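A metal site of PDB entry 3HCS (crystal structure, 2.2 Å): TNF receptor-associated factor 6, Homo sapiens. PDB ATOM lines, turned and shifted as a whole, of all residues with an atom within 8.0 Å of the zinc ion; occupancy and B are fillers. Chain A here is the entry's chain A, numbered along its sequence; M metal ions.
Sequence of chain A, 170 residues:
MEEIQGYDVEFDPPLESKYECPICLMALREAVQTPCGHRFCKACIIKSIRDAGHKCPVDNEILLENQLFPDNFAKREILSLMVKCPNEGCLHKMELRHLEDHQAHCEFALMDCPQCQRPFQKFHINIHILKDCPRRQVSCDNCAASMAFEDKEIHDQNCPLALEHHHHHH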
ATOM      1  N   LYS A  84      22.435  -4.864 -17.617  1.00  0.00           N
ATOM      2  CA  LYS A  84      21.469  -5.589 -16.807  1.00  0.00           C
ATOM      3  C   LYS A  84      22.089  -6.913 -16.380  1.00  0.00           C
ATOM      4  O   LYS A  84      22.825  -7.533 -17.151  1.00  0.00           O
ATOM      5  CB  LYS A  84      20.181  -5.840 -17.588  1.00  0.00           C
ATOM      6  CG  LYS A  84      19.488  -4.566 -18.023  1.00  0.00           C
ATOM      7  CD  LYS A  84      17.992  -4.740 -18.183  1.00  0.00           C
ATOM      8  CE  LYS A  84      17.647  -5.686 -19.313  1.00  0.00           C
ATOM      9  NZ  LYS A  84      16.177  -5.918 -19.366  1.00  0.00           N
ATOM     10  N   CYS A  85      21.811  -7.343 -15.153  1.00  0.00           N
ATOM     11  CA  CYS A  85      22.343  -8.615 -14.677  1.00  0.00           C
ATOM     12  C   CYS A  85      21.706  -9.732 -15.473  1.00  0.00           C
ATOM     13  O   CYS A  85      20.487  -9.763 -15.644  1.00  0.00           O
ATOM     14  CB  CYS A  85      22.035  -8.792 -13.191  1.00  0.00           C
ATOM     15  SG  CYS A  85      22.420 -10.444 -12.593  1.00  0.00           S
ATOM     16  N   PRO A  86      22.520 -10.681 -15.976  1.00  0.00           N
ATOM     17  CA  PRO A  86      22.024 -11.814 -16.764  1.00  0.00           C
ATOM     18  C   PRO A  86      21.187 -12.829 -15.986  1.00  0.00           C
ATOM     19  O   PRO A  86      20.272 -13.453 -16.557  1.00  0.00           O
ATOM     20  CB  PRO A  86      23.299 -12.426 -17.324  1.00  0.00           C
ATOM     21  CG  PRO A  86      24.271 -12.215 -16.210  1.00  0.00           C
ATOM     22  CD  PRO A  86      23.990 -10.761 -15.828  1.00  0.00           C
ATOM     23  N   ASN A  87      21.437 -12.974 -14.695  1.00  0.00           N
ATOM     24  CA  ASN A  87      20.712 -13.949 -13.889  1.00  0.00           C
ATOM     25  C   ASN A  87      19.204 -13.843 -13.936  1.00  0.00           C
ATOM     26  O   ASN A  87      18.632 -12.767 -13.737  1.00  0.00           O
ATOM     27  CB  ASN A  87      21.170 -13.897 -12.437  1.00  0.00           C
ATOM     28  CG  ASN A  87      22.648 -14.127 -12.291  1.00  0.00           C
ATOM     29  OD1 ASN A  87      23.233 -14.936 -13.012  1.00  0.00           O
ATOM     30  ND2 ASN A  87      23.267 -13.412 -11.363  1.00  0.00           N
ATOM     31  N   GLU A  88      18.560 -14.974 -14.173  1.00  0.00           N
ATOM     32  CA  GLU A  88      17.107 -15.025 -14.247  1.00  0.00           C
ATOM     33  C   GLU A  88      16.453 -14.622 -12.937  1.00  0.00           C
ATOM     34  O   GLU A  88      16.768 -15.145 -11.875  1.00  0.00           O
ATOM     35  CB  GLU A  88      16.648 -16.438 -14.630  1.00  0.00           C
ATOM     36  CG  GLU A  88      15.140 -16.588 -14.753  1.00  0.00           C
ATOM     37  CD  GLU A  88      14.523 -15.596 -15.727  1.00  0.00           C
ATOM     38  OE1 GLU A  88      15.057 -15.438 -16.839  1.00  0.00           O
ATOM     39  OE2 GLU A  88      13.495 -14.966 -15.371  1.00  0.00           O
ATOM     40  N   GLY A  89      15.526 -13.677 -13.024  1.00  0.00           N
ATOM     41  CA  GLY A  89      14.848 -13.200 -11.835  1.00  0.00           C
ATOM     42  C   GLY A  89      15.418 -11.874 -11.349  1.00  0.00           C
ATOM     43  O   GLY A  89      14.700 -11.087 -10.720  1.00  0.00           O
ATOM     44  N   CYS A  90      16.688 -11.614 -11.622  1.00  0.00           N
ATOM     45  CA  CYS A  90      17.299 -10.377 -11.158  1.00  0.00           C
ATOM     46  C   CYS A  90      16.916  -9.188 -12.027  1.00  0.00           C
ATOM     47  O   CYS A  90      16.845  -9.281 -13.246  1.00  0.00           O
ATOM     48  CB  CYS A  90      18.826 -10.494 -11.101  1.00  0.00           C
ATOM     49  SG  CYS A  90      19.614  -9.078 -10.270  1.00  0.00           S
ATOM     50  N   LEU A  91      16.666  -8.052 -11.375  1.00  0.00           N
ATOM     51  CA  LEU A  91      16.286  -6.851 -12.091  1.00  0.00           C
ATOM     52  C   LEU A  91      17.286  -5.726 -11.886  1.00  0.00           C
ATOM     53  O   LEU A  91      17.013  -4.573 -12.227  1.00  0.00           O
ATOM     54  CB  LEU A  91      14.902  -6.383 -11.625  1.00  0.00           C
ATOM     55  CG  LEU A  91      13.646  -7.165 -12.026  1.00  0.00           C
ATOM     56  CD1 LEU A  91      12.449  -6.652 -11.210  1.00  0.00           C
ATOM     57  CD2 LEU A  91      13.368  -6.993 -13.530  1.00  0.00           C
ATOM     58  N   HIS A  92      18.436  -6.044 -11.288  1.00  0.00           N
ATOM     59  CA  HIS A  92      19.456  -5.021 -11.058  1.00  0.00           C
ATOM     60  C   HIS A  92      20.126  -4.562 -12.353  1.00  0.00           C
ATOM     61  O   HIS A  92      20.353  -5.348 -13.275  1.00  0.00           O
ATOM     62  CB  HIS A  92      20.503  -5.548 -10.088  1.00  0.00           C
ATOM     63  CG  HIS A  92      20.057  -5.588  -8.663  1.00  0.00           C
ATOM     64  ND1 HIS A  92      19.674  -4.457  -7.972  1.00  0.00           N
ATOM     65  CD2 HIS A  92      19.931  -6.612  -7.795  1.00  0.00           C
ATOM     66  CE1 HIS A  92      19.335  -4.790  -6.742  1.00  0.00           C
ATOM     67  NE2 HIS A  92      19.488  -6.096  -6.605  1.00  0.00           N
ATOM     68  N   LYS A  93      20.395  -3.268 -12.426  1.00  0.00           N
ATOM     69  CA  LYS A  93      21.072  -2.644 -13.557  1.00  0.00           C
ATOM     70  C   LYS A  93      22.229  -1.912 -12.922  1.00  0.00           C
ATOM     71  O   LYS A  93      22.063  -1.310 -11.864  1.00  0.00           O
ATOM     72  CB  LYS A  93      20.189  -1.591 -14.253  1.00  0.00           C
ATOM     73  CG  LYS A  93      19.034  -2.114 -15.072  1.00  0.00           C
ATOM     74  CD  LYS A  93      18.383  -0.933 -15.790  1.00  0.00           C
ATOM     75  CE  LYS A  93      17.354  -1.381 -16.811  1.00  0.00           C
ATOM     76  NZ  LYS A  93      16.841  -0.212 -17.585  1.00  0.00           N
ATOM     77  N   MET A  94      23.402  -1.940 -13.553  1.00  0.00           N
ATOM     78  CA  MET A  94      24.562  -1.270 -12.984  1.00  0.00           C
ATOM     79  C   MET A  94      25.570  -0.968 -14.081  1.00  0.00           C
ATOM     80  O   MET A  94      25.380  -1.394 -15.215  1.00  0.00           O
ATOM     81  CB  MET A  94      25.216  -2.201 -11.959  1.00  0.00           C
ATOM     82  CG  MET A  94      25.707  -3.507 -12.596  1.00  0.00           C
ATOM     83  SD  MET A  94      25.495  -4.971 -11.587  1.00  0.00           S
ATOM     84  CE  MET A  94      23.717  -5.256 -11.775  1.00  0.00           C
ATOM     85  N   LEU A  99      29.590  -5.151 -12.663  1.00  0.00           N
ATOM     86  CA  LEU A  99      28.885  -6.419 -12.897  1.00  0.00           C
ATOM     87  C   LEU A  99      29.585  -7.656 -12.337  1.00  0.00           C
ATOM     88  O   LEU A  99      28.931  -8.552 -11.823  1.00  0.00           O
ATOM     89  CB  LEU A  99      28.619  -6.616 -14.386  1.00  0.00           C
ATOM     90  CG  LEU A  99      27.869  -7.911 -14.744  1.00  0.00           C
ATOM     91  CD1 LEU A  99      26.450  -7.871 -14.168  1.00  0.00           C
ATOM     92  CD2 LEU A  99      27.822  -8.084 -16.257  1.00  0.00           C
ATOM     93  N   HIS A 102      29.129  -7.866  -8.663  1.00  0.00           N
ATOM     94  CA  HIS A 102      27.730  -8.187  -8.430  1.00  0.00           C
ATOM     95  C   HIS A 102      27.387  -9.661  -8.581  1.00  0.00           C
ATOM     96  O   HIS A 102      26.670 -10.230  -7.762  1.00  0.00           O
ATOM     97  CB  HIS A 102      26.837  -7.387  -9.379  1.00  0.00           C
ATOM     98  CG  HIS A 102      25.392  -7.776  -9.299  1.00  0.00           C
ATOM     99  ND1 HIS A 102      24.600  -7.460  -8.230  1.00  0.00           N
ATOM    100  CD2 HIS A 102      24.621  -8.509 -10.140  1.00  0.00           C
ATOM    101  CE1 HIS A 102      23.388  -7.972  -8.407  1.00  0.00           C
ATOM    102  NE2 HIS A 102      23.386  -8.611  -9.559  1.00  0.00           N
ATOM    103  N   GLN A 103      27.872 -10.248  -9.663  1.00  0.00           N
ATOM    104  CA  GLN A 103      27.605 -11.659  -9.946  1.00  0.00           C
ATOM    105  C   GLN A 103      28.084 -12.574  -8.840  1.00  0.00           C
ATOM    106  O   GLN A 103      27.507 -13.635  -8.614  1.00  0.00           O
ATOM    107  CB  GLN A 103      28.251 -12.046 -11.280  1.00  0.00           C
ATOM    108  CG  GLN A 103      28.249 -13.551 -11.591  1.00  0.00           C
ATOM    109  CD  GLN A 103      26.853 -14.169 -11.716  1.00  0.00           C
ATOM    110  OE1 GLN A 103      25.857 -13.468 -11.885  1.00  0.00           O
ATOM    111  NE2 GLN A 103      26.793 -15.494 -11.641  1.00  0.00           N
ATOM    112  N   ALA A 104      29.135 -12.167  -8.123  1.00  0.00           N
ATOM    113  CA  ALA A 104      29.665 -12.982  -7.040  1.00  0.00           C
ATOM    114  C   ALA A 104      28.743 -12.970  -5.830  1.00  0.00           C
ATOM    115  O   ALA A 104      28.863 -13.816  -4.948  1.00  0.00           O
ATOM    116  CB  ALA A 104      31.069 -12.499  -6.650  1.00  0.00           C
ATOM    117  N   HIS A 105      27.803 -12.023  -5.811  1.00  0.00           N
ATOM    118  CA  HIS A 105      26.875 -11.919  -4.689  1.00  0.00           C
ATOM    119  C   HIS A 105      25.406 -12.041  -5.085  1.00  0.00           C
ATOM    120  O   HIS A 105      24.541 -12.184  -4.216  1.00  0.00           O
ATOM    121  CB  HIS A 105      27.064 -10.582  -3.958  1.00  0.00           C
ATOM    122  CG  HIS A 105      28.447 -10.382  -3.426  1.00  0.00           C
ATOM    123  ND1 HIS A 105      29.115 -11.343  -2.707  1.00  0.00           N
ATOM    124  CD2 HIS A 105      29.273  -9.312  -3.487  1.00  0.00           C
ATOM    125  CE1 HIS A 105      30.307 -10.882  -2.357  1.00  0.00           C
ATOM    126  NE2 HIS A 105      30.425  -9.642  -2.823  1.00  0.00           N
ATOM    127  N   CYS A 106      25.114 -11.994  -6.376  1.00  0.00           N
ATOM    128  CA  CYS A 106      23.720 -12.085  -6.832  1.00  0.00           C
ATOM    129  C   CYS A 106      23.008 -13.326  -6.343  1.00  0.00           C
ATOM    130  O   CYS A 106      23.474 -14.459  -6.554  1.00  0.00           O
ATOM    131  CB  CYS A 106      23.638 -12.033  -8.360  1.00  0.00           C
ATOM    132  SG  CYS A 106      21.917 -12.026  -8.958  1.00  0.00           S
ATOM    133  N   GLU A 107      21.852 -13.130  -5.706  1.00  0.00           N
ATOM    134  CA  GLU A 107      21.091 -14.247  -5.150  1.00  0.00           C
ATOM    135  C   GLU A 107      20.371 -15.047  -6.220  1.00  0.00           C
ATOM    136  O   GLU A 107      19.713 -16.035  -5.910  1.00  0.00           O
ATOM    137  CB  GLU A 107      20.090 -13.755  -4.092  1.00  0.00           C
ATOM    138  CG  GLU A 107      19.145 -12.639  -4.547  1.00  0.00           C
ATOM    139  CD  GLU A 107      19.738 -11.246  -4.394  1.00  0.00           C
ATOM    140  OE1 GLU A 107      20.939 -11.061  -4.680  1.00  0.00           O
ATOM    141  OE2 GLU A 107      19.006 -10.312  -3.991  1.00  0.00           O
ATOM    142  N   PHE A 108      20.472 -14.622  -7.475  1.00  0.00           N
ATOM    143  CA  PHE A 108      19.813 -15.332  -8.556  1.00  0.00           C
ATOM    144  C   PHE A 108      20.784 -16.166  -9.393  1.00  0.00           C
ATOM    145  O   PHE A 108      20.358 -16.843 -10.314  1.00  0.00           O
ATOM    146  CB  PHE A 108      19.053 -14.360  -9.444  1.00  0.00           C
ATOM    147  CG  PHE A 108      17.859 -13.742  -8.771  1.00  0.00           C
ATOM    148  CD1 PHE A 108      16.655 -14.436  -8.702  1.00  0.00           C
ATOM    149  CD2 PHE A 108      17.948 -12.491  -8.183  1.00  0.00           C
ATOM    150  CE1 PHE A 108      15.549 -13.876  -8.056  1.00  0.00           C
ATOM    151  CE2 PHE A 108      16.845 -11.918  -7.530  1.00  0.00           C
ATOM    152  CZ  PHE A 108      15.649 -12.617  -7.471  1.00  0.00           C
ATOM    153  N   ALA A 109      22.068 -16.128  -9.044  1.00  0.00           N
ATOM    154  CA  ALA A 109      23.085 -16.883  -9.761  1.00  0.00           C
ATOM    155  C   ALA A 109      22.936 -18.368  -9.423  1.00  0.00           C
ATOM    156  O   ALA A 109      22.619 -18.711  -8.287  1.00  0.00           O
ATOM    157  CB  ALA A 109      24.459 -16.396  -9.378  1.00  0.00           C
HETATM  158 ZN    ZN M   1      21.776  -9.976 -10.269  1.00  0.00          ZN
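ND2 of Asn 87 touches the zinc ion (3.9 Å). The nearest printed residue that does not touch the zinc ion is His 92 (4.6 Å).
N of His 92 sits close to SG of Cys 90 (3.4 Å). The backbone NH (N) of Cys 85 is in hydrogen-bond range of the backbone carbonyl oxygen (O) of His 92 (3.1 Å). OE1 of Gln 103 lies within hydrogen-bond range of ND2 of Asn 87, at 2.6 Å. N of Phe 108 lies close to SG of Cys 106 (3.3 Å). The side-chain sulfur of Cys 106 lies close to the side-chain amide nitrogen of Asn 87, 3.1 Å away. SG of Cys 85 sits close to ND2 of Asn 87 (3.3 Å).
A ring nitrogen (NE2) of His 102 is bound to the zinc ion, at 2.2 Å. SG of Cys 90 binds the zinc ion, at 2.3 Å. SG of Cys 106 binds the zinc ion (2.4 Å). SG of Cys 85 binds the zinc ion (2.5 Å).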
